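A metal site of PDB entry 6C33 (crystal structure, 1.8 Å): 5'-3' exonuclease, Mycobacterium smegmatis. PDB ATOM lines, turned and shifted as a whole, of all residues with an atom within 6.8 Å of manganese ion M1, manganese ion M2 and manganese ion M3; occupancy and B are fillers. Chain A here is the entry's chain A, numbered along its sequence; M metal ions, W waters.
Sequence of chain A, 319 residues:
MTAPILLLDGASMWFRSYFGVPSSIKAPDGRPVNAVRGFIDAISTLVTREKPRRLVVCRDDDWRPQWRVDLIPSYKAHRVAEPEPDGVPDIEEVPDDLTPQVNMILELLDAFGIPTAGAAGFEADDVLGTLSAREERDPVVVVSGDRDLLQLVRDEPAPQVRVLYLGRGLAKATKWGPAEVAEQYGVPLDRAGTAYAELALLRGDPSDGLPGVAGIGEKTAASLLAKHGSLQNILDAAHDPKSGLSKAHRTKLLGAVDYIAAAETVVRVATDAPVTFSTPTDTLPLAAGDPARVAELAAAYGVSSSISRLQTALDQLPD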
ATOM      1  N   ASP A   9     -33.766   2.226  19.599  1.00  0.00           N
ATOM      2  CA  ASP A   9     -33.028   3.198  20.425  1.00  0.00           C
ATOM      3  C   ASP A   9     -32.209   4.041  19.456  1.00  0.00           C
ATOM      4  O   ASP A   9     -31.093   3.671  19.088  1.00  0.00           O
ATOM      5  CB  ASP A   9     -32.160   2.471  21.442  1.00  0.00           C
ATOM      6  CG  ASP A   9     -31.444   3.413  22.399  1.00  0.00           C
ATOM      7  OD1 ASP A   9     -31.400   4.634  22.173  1.00  0.00           O
ATOM      8  OD2 ASP A   9     -30.893   2.872  23.381  1.00  0.00           O
ATOM      9  N   ALA A  11     -30.421   6.890  19.305  1.00  0.00           N
ATOM     10  CA  ALA A  11     -29.073   7.376  19.565  1.00  0.00           C
ATOM     11  C   ALA A  11     -28.106   6.217  19.756  1.00  0.00           C
ATOM     12  O   ALA A  11     -26.939   6.306  19.349  1.00  0.00           O
ATOM     13  CB  ALA A  11     -29.079   8.289  20.785  1.00  0.00           C
ATOM     14  N   SER A  12     -28.546   5.133  20.377  1.00  0.00           N
ATOM     15  CA  SER A  12     -27.677   3.956  20.432  1.00  0.00           C
ATOM     16  C   SER A  12     -27.265   3.540  19.033  1.00  0.00           C
ATOM     17  O   SER A  12     -26.081   3.294  18.772  1.00  0.00           O
ATOM     18  CB  SER A  12     -28.384   2.794  21.150  1.00  0.00           C
ATOM     19  OG  SER A  12     -27.556   1.639  21.080  1.00  0.00           O
ATOM     20  N   ASP A  60     -34.352  10.898  22.188  1.00  0.00           N
ATOM     21  CA  ASP A  60     -33.940  11.486  23.461  1.00  0.00           C
ATOM     22  C   ASP A  60     -34.364  12.957  23.455  1.00  0.00           C
ATOM     23  O   ASP A  60     -33.597  13.839  23.094  1.00  0.00           O
ATOM     24  CB  ASP A  60     -32.432  11.369  23.635  1.00  0.00           C
ATOM     25  CG  ASP A  60     -31.985   9.983  24.017  1.00  0.00           C
ATOM     26  OD1 ASP A  60     -31.517   9.222  23.120  1.00  0.00           O
ATOM     27  OD2 ASP A  60     -32.121   9.661  25.207  1.00  0.00           O
ATOM     28  N   TRP A  63     -31.603  13.812  26.772  1.00  0.00           N
ATOM     29  CA  TRP A  63     -30.674  12.704  26.988  1.00  0.00           C
ATOM     30  C   TRP A  63     -30.191  12.605  28.436  1.00  0.00           C
ATOM     31  O   TRP A  63     -29.714  11.538  28.827  1.00  0.00           O
ATOM     32  CB  TRP A  63     -29.467  12.836  26.067  1.00  0.00           C
ATOM     33  CG  TRP A  63     -28.557  13.940  26.483  1.00  0.00           C
ATOM     34  CD1 TRP A  63     -28.739  15.276  26.294  1.00  0.00           C
ATOM     35  CD2 TRP A  63     -27.315  13.804  27.193  1.00  0.00           C
ATOM     36  NE1 TRP A  63     -27.680  15.985  26.829  1.00  0.00           N
ATOM     37  CE2 TRP A  63     -26.798  15.103  27.387  1.00  0.00           C
ATOM     38  CE3 TRP A  63     -26.589  12.703  27.685  1.00  0.00           C
ATOM     39  CZ2 TRP A  63     -25.594  15.337  28.057  1.00  0.00           C
ATOM     40  CZ3 TRP A  63     -25.398  12.940  28.344  1.00  0.00           C
ATOM     41  CH2 TRP A  63     -24.906  14.247  28.515  1.00  0.00           C
ATOM     42  N   TYR A  75     -24.716  11.412  37.527  1.00  0.00           N
ATOM     43  CA  TYR A  75     -25.368  10.733  36.415  1.00  0.00           C
ATOM     44  C   TYR A  75     -25.017  11.394  35.095  1.00  0.00           C
ATOM     45  O   TYR A  75     -25.384  12.544  34.856  1.00  0.00           O
ATOM     46  CB  TYR A  75     -26.880  10.743  36.631  1.00  0.00           C
ATOM     47  CG  TYR A  75     -27.646  10.022  35.554  1.00  0.00           C
ATOM     48  CD1 TYR A  75     -27.554   8.663  35.427  1.00  0.00           C
ATOM     49  CD2 TYR A  75     -28.464  10.731  34.661  1.00  0.00           C
ATOM     50  CE1 TYR A  75     -28.263   7.980  34.442  1.00  0.00           C
ATOM     51  CE2 TYR A  75     -29.174  10.070  33.675  1.00  0.00           C
ATOM     52  CZ  TYR A  75     -29.075   8.696  33.580  1.00  0.00           C
ATOM     53  OH  TYR A  75     -29.787   8.015  32.625  1.00  0.00           O
ATOM     54  N   LYS A  76     -24.319  10.640  34.234  1.00  0.00           N
ATOM     55  CA  LYS A  76     -23.873  11.068  32.907  1.00  0.00           C
ATOM     56  C   LYS A  76     -23.035  12.341  32.934  1.00  0.00           C
ATOM     57  O   LYS A  76     -22.848  12.974  31.897  1.00  0.00           O
ATOM     58  CB  LYS A  76     -25.053  11.253  31.947  1.00  0.00           C
ATOM     59  CG  LYS A  76     -25.803   9.953  31.677  1.00  0.00           C
ATOM     60  CD  LYS A  76     -26.857  10.120  30.587  1.00  0.00           C
ATOM     61  CE  LYS A  76     -27.527   8.777  30.285  1.00  0.00           C
ATOM     62  NZ  LYS A  76     -28.290   8.821  29.003  1.00  0.00           N
ATOM     63  N   ARG A  79     -20.148  12.886  30.463  1.00  0.00           N
ATOM     64  CA  ARG A  79     -20.498  13.009  29.053  1.00  0.00           C
ATOM     65  C   ARG A  79     -21.054  14.365  28.685  1.00  0.00           C
ATOM     66  O   ARG A  79     -21.481  14.557  27.536  1.00  0.00           O
ATOM     67  CB  ARG A  79     -21.518  11.922  28.668  1.00  0.00           C
ATOM     68  CG  ARG A  79     -20.987  10.514  28.878  1.00  0.00           C
ATOM     69  CD  ARG A  79     -21.781   9.517  28.080  1.00  0.00           C
ATOM     70  NE  ARG A  79     -22.595   8.674  28.918  1.00  0.00           N
ATOM     71  CZ  ARG A  79     -23.751   8.148  28.544  1.00  0.00           C
ATOM     72  NH1 ARG A  79     -24.236   8.393  27.327  1.00  0.00           N
ATOM     73  NH2 ARG A  79     -24.435   7.380  29.376  1.00  0.00           N
ATOM     74  N   GLU A 123     -35.606  10.360  28.561  1.00  0.00           N
ATOM     75  CA  GLU A 123     -34.655   9.707  27.680  1.00  0.00           C
ATOM     76  C   GLU A 123     -35.381   8.762  26.733  1.00  0.00           C
ATOM     77  O   GLU A 123     -36.512   8.324  26.967  1.00  0.00           O
ATOM     78  CB  GLU A 123     -33.647   8.915  28.481  1.00  0.00           C
ATOM     79  CG  GLU A 123     -32.796   9.770  29.373  1.00  0.00           C
ATOM     80  CD  GLU A 123     -31.733   8.985  30.097  1.00  0.00           C
ATOM     81  OE1 GLU A 123     -31.064   8.140  29.461  1.00  0.00           O
ATOM     82  OE2 GLU A 123     -31.549   9.229  31.308  1.00  0.00           O
ATOM     83  N   ALA A 124     -34.690   8.417  25.640  1.00  0.00           N
ATOM     84  CA  ALA A 124     -35.237   7.378  24.773  1.00  0.00           C
ATOM     85  C   ALA A 124     -35.409   6.085  25.547  1.00  0.00           C
ATOM     86  O   ALA A 124     -36.348   5.320  25.286  1.00  0.00           O
ATOM     87  CB  ALA A 124     -34.335   7.180  23.553  1.00  0.00           C
ATOM     88  N   ASP A 125     -34.541   5.850  26.550  1.00  0.00           N
ATOM     89  CA  ASP A 125     -34.701   4.684  27.407  1.00  0.00           C
ATOM     90  C   ASP A 125     -36.093   4.629  28.027  1.00  0.00           C
ATOM     91  O   ASP A 125     -36.703   3.561  28.122  1.00  0.00           O
ATOM     92  CB  ASP A 125     -33.653   4.684  28.515  1.00  0.00           C
ATOM     93  CG  ASP A 125     -32.237   4.818  28.001  1.00  0.00           C
ATOM     94  OD1 ASP A 125     -32.010   5.506  26.972  1.00  0.00           O
ATOM     95  OD2 ASP A 125     -31.339   4.235  28.649  1.00  0.00           O
ATOM     96  N   LEU A 128     -38.786   3.953  25.325  1.00  0.00           N
ATOM     97  CA  LEU A 128     -38.773   2.517  25.058  1.00  0.00           C
ATOM     98  C   LEU A 128     -39.489   1.750  26.159  1.00  0.00           C
ATOM     99  O   LEU A 128     -40.315   0.872  25.883  1.00  0.00           O
ATOM    100  CB  LEU A 128     -37.322   2.044  24.902  1.00  0.00           C
ATOM    101  CG  LEU A 128     -36.647   2.547  23.626  1.00  0.00           C
ATOM    102  CD1 LEU A 128     -35.116   2.477  23.718  1.00  0.00           C
ATOM    103  CD2 LEU A 128     -37.118   1.736  22.436  1.00  0.00           C
ATOM    104  N   SER A 144     -31.201  -2.065  20.631  1.00  0.00           N
ATOM    105  CA  SER A 144     -30.318  -1.125  21.318  1.00  0.00           C
ATOM    106  C   SER A 144     -29.013  -1.813  21.710  1.00  0.00           C
ATOM    107  O   SER A 144     -28.994  -3.008  21.989  1.00  0.00           O
ATOM    108  CB  SER A 144     -30.978  -0.566  22.589  1.00  0.00           C
ATOM    109  OG  SER A 144     -30.106   0.353  23.236  1.00  0.00           O
ATOM    110  N   ASP A 146     -27.532  -0.528  24.414  1.00  0.00           N
ATOM    111  CA  ASP A 146     -27.464  -0.065  25.803  1.00  0.00           C
ATOM    112  C   ASP A 146     -28.022  -1.156  26.707  1.00  0.00           C
ATOM    113  O   ASP A 146     -29.208  -1.485  26.628  1.00  0.00           O
ATOM    114  CB  ASP A 146     -28.261   1.224  25.935  1.00  0.00           C
ATOM    115  CG  ASP A 146     -28.269   1.796  27.331  1.00  0.00           C
ATOM    116  OD1 ASP A 146     -27.656   1.224  28.259  1.00  0.00           O
ATOM    117  OD2 ASP A 146     -28.921   2.859  27.510  1.00  0.00           O
ATOM    118  N   ARG A 147     -27.166  -1.714  27.571  1.00  0.00           N
ATOM    119  CA  ARG A 147     -27.647  -2.779  28.458  1.00  0.00           C
ATOM    120  C   ARG A 147     -28.703  -2.301  29.446  1.00  0.00           C
ATOM    121  O   ARG A 147     -29.405  -3.150  30.021  1.00  0.00           O
ATOM    122  CB  ARG A 147     -26.466  -3.400  29.219  1.00  0.00           C
ATOM    123  CG  ARG A 147     -25.666  -4.359  28.389  1.00  0.00           C
ATOM    124  CD  ARG A 147     -24.487  -4.888  29.173  1.00  0.00           C
ATOM    125  NE  ARG A 147     -23.676  -3.819  29.735  1.00  0.00           N
ATOM    126  CZ  ARG A 147     -22.384  -3.939  30.045  1.00  0.00           C
ATOM    127  NH1 ARG A 147     -21.758  -5.085  29.850  1.00  0.00           N
ATOM    128  NH2 ARG A 147     -21.731  -2.909  30.549  1.00  0.00           N
ATOM    129  N   ASP A 148     -28.863  -0.991  29.641  1.00  0.00           N
ATOM    130  CA  ASP A 148     -29.979  -0.495  30.452  1.00  0.00           C
ATOM    131  C   ASP A 148     -31.298  -1.118  30.033  1.00  0.00           C
ATOM    132  O   ASP A 148     -32.180  -1.333  30.872  1.00  0.00           O
ATOM    133  CB  ASP A 148     -30.131   1.021  30.332  1.00  0.00           C
ATOM    134  CG  ASP A 148     -28.998   1.800  30.968  1.00  0.00           C
ATOM    135  OD1 ASP A 148     -28.247   1.229  31.795  1.00  0.00           O
ATOM    136  OD2 ASP A 148     -28.856   3.012  30.629  1.00  0.00           O
ATOM    137  N   LEU A 149     -31.463  -1.394  28.745  1.00  0.00           N
ATOM    138  CA  LEU A 149     -32.766  -1.845  28.285  1.00  0.00           C
ATOM    139  C   LEU A 149     -33.010  -3.317  28.565  1.00  0.00           C
ATOM    140  O   LEU A 149     -34.139  -3.777  28.369  1.00  0.00           O
ATOM    141  CB  LEU A 149     -32.942  -1.529  26.813  1.00  0.00           C
ATOM    142  CG  LEU A 149     -32.926   0.007  26.733  1.00  0.00           C
ATOM    143  CD1 LEU A 149     -32.715   0.459  25.358  1.00  0.00           C
ATOM    144  CD2 LEU A 149     -34.222   0.612  27.292  1.00  0.00           C
ATOM    145  N   ASP A 205     -22.708   1.506  37.338  1.00  0.00           N
ATOM    146  CA  ASP A 205     -22.913   1.699  35.903  1.00  0.00           C
ATOM    147  C   ASP A 205     -21.939   2.777  35.461  1.00  0.00           C
ATOM    148  O   ASP A 205     -22.268   3.970  35.452  1.00  0.00           O
ATOM    149  CB  ASP A 205     -24.355   2.095  35.613  1.00  0.00           C
ATOM    150  CG  ASP A 205     -24.678   2.168  34.127  1.00  0.00           C
ATOM    151  OD1 ASP A 205     -23.767   2.171  33.276  1.00  0.00           O
ATOM    152  OD2 ASP A 205     -25.881   2.244  33.827  1.00  0.00           O
ATOM    153  N   SER A 207     -20.596   3.685  32.564  1.00  0.00           N
ATOM    154  CA  SER A 207     -20.902   4.508  31.398  1.00  0.00           C
ATOM    155  C   SER A 207     -21.904   5.614  31.720  1.00  0.00           C
ATOM    156  O   SER A 207     -21.868   6.677  31.093  1.00  0.00           O
ATOM    157  CB  SER A 207     -21.411   3.637  30.239  1.00  0.00           C
ATOM    158  OG  SER A 207     -22.337   2.663  30.687  1.00  0.00           O
ATOM    159  N   ASP A 208     -22.792   5.400  32.699  1.00  0.00           N
ATOM    160  CA  ASP A 208     -23.720   6.441  33.112  1.00  0.00           C
ATOM    161  C   ASP A 208     -23.252   7.211  34.345  1.00  0.00           C
ATOM    162  O   ASP A 208     -23.990   8.044  34.877  1.00  0.00           O
ATOM    163  CB  ASP A 208     -25.104   5.836  33.370  1.00  0.00           C
ATOM    164  CG  ASP A 208     -25.957   5.725  32.103  1.00  0.00           C
ATOM    165  OD1 ASP A 208     -25.519   6.174  31.015  1.00  0.00           O
ATOM    166  OD2 ASP A 208     -27.071   5.193  32.214  1.00  0.00           O
ATOM    167  N   LEU A 210     -22.699   6.123  37.447  1.00  0.00           N
ATOM    168  CA  LEU A 210     -23.337   5.704  38.699  1.00  0.00           C
ATOM    169  C   LEU A 210     -22.392   4.797  39.464  1.00  0.00           C
ATOM    170  O   LEU A 210     -22.050   3.724  38.952  1.00  0.00           O
ATOM    171  CB  LEU A 210     -24.646   4.987  38.408  1.00  0.00           C
ATOM    172  CG  LEU A 210     -25.675   5.859  37.711  1.00  0.00           C
ATOM    173  CD1 LEU A 210     -26.871   5.036  37.265  1.00  0.00           C
ATOM    174  CD2 LEU A 210     -26.097   7.017  38.643  1.00  0.00           C
ATOM    175  N   VAL A 267     -32.136   4.531  37.959  1.00  0.00           N
ATOM    176  CA  VAL A 267     -31.742   3.352  37.167  1.00  0.00           C
ATOM    177  C   VAL A 267     -32.931   2.759  36.423  1.00  0.00           C
ATOM    178  O   VAL A 267     -32.787   2.282  35.282  1.00  0.00           O
ATOM    179  CB  VAL A 267     -31.074   2.315  38.102  1.00  0.00           C
ATOM    180  CG1 VAL A 267     -30.878   0.989  37.388  1.00  0.00           C
ATOM    181  CG2 VAL A 267     -29.743   2.841  38.610  1.00  0.00           C
ATOM    182  N   VAL A 269     -36.061   2.594  34.136  1.00  0.00           N
ATOM    183  CA  VAL A 269     -36.653   3.398  33.072  1.00  0.00           C
ATOM    184  C   VAL A 269     -38.108   3.688  33.432  1.00  0.00           C
ATOM    185  O   VAL A 269     -38.803   2.845  34.027  1.00  0.00           O
ATOM    186  CB  VAL A 269     -36.538   2.702  31.703  1.00  0.00           C
ATOM    187  CG1 VAL A 269     -35.092   2.338  31.428  1.00  0.00           C
ATOM    188  CG2 VAL A 269     -37.415   1.464  31.661  1.00  0.00           C
HETATM  189 MN    MN M   1     -29.187   4.387  28.969  1.00  0.00          MN
HETATM  190 MN    MN M   2     -30.098   6.203  25.960  1.00  0.00          MN
HETATM  191 MN    MN M   3     -27.288   3.071  32.372  1.00  0.00          MN
HETATM  192  O   HOH W   1     -28.910   3.535  33.773  1.00  0.00           O
HETATM  193  O   HOH W   2     -25.868   2.506  31.186  1.00  0.00           O
HETATM  194  O   HOH W   3     -30.580   8.190  26.637  1.00  0.00           O
HETATM  195  O   HOH W   4     -31.014   6.596  24.038  1.00  0.00           O
HETATM  196  O   HOH W   5     -29.001   5.869  27.588  1.00  0.00           O
HETATM  197  O   HOH W   6     -26.944   4.755  28.998  1.00  0.00           O
HETATM  198  O   HOH W   7     -29.638   4.171  25.275  1.00  0.00           O
HETATM  199  O   HOH W   8     -29.494   5.936  30.614  1.00  0.00           O
HETATM  200  O   HOH W   9     -28.143   6.982  25.085  1.00  0.00           O
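OG of Ser 144 sits at hydrogen-bond distance from N of Asp 146 (3.0 Å). O of Asp 208 lies within hydrogen-bond range of N of Lys 76, 2.7 Å away. The side-chain hydroxyl (OG) of Ser 207 sits at hydrogen-bond distance from the side-chain carboxylate (OD1) of Asp 205 (3.0 Å). N of Asp 205 is in hydrogen-bond range of O of Leu 210 (2.8 Å).
Along chain A the residues within 4 Å of manganese ion M1 span positions 125 to 208. The nearest printed residue that does not touch manganese ion M1 is Glu 123 (4.2 Å).
Two residues have an atom within 4 Å of manganese ion M2: Asp 125 and Asp 146. The nearest printed residue that does not touch manganese ion M2 is Asp 60 (4.1 Å).
Of the 23 residues printed, 3 come within 4 Å of manganese ion M3. The nearest printed residue that does not touch manganese ion M3 is Asp 146 (4.5 Å).
Manganese ion M1 is bound by water W5 (2.0 Å), OD2 of Asp 146 (2.1 Å), OD2 of Asp 148 (2.2 Å), OD2 of Asp 125 (2.2 Å), water W6 (2.3 Å) and water W8 (2.3 Å). Manganese ion M1 has six donor atoms within binding distance.
Manganese ion M2 is bound by water W5 (2.0 Å), water W3 (2.2 Å), water W4 (2.2 Å), water W7 (2.2 Å), the side-chain carboxylate of Asp 125 (2.3 Å) and water W9 (2.3 Å).
Manganese ion M3 is bound by water W2 (1.9 Å), the side-chain carboxylate (OD2) of Asp 208 (2.1 Å), the side-chain carboxylate (OD1) of Asp 148 (2.2 Å), the side-chain carboxylate (OD2) of Asp 205 (2.2 Å), water W1 (2.2 Å) and the side-chain carboxylate (OD2) of Asp 148 (2.3 Å).
Water W8 lies within hydrogen-bond range of OH of Tyr 75 (2.9 Å) and OE1 of Glu 123 (2.9 Å). Water W4 bridges the side-chain carboxylate (OD1) of Asp 9 (2.7 Å) and the side-chain carboxylate (OD1) of Asp 60 (2.8 Å). Water W3 lies within hydrogen-bond range of OD2 of Asp 60 (2.6 Å), OE1 of Glu 123 (2.9 Å) and NZ of Lys 76 (3.4 Å).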
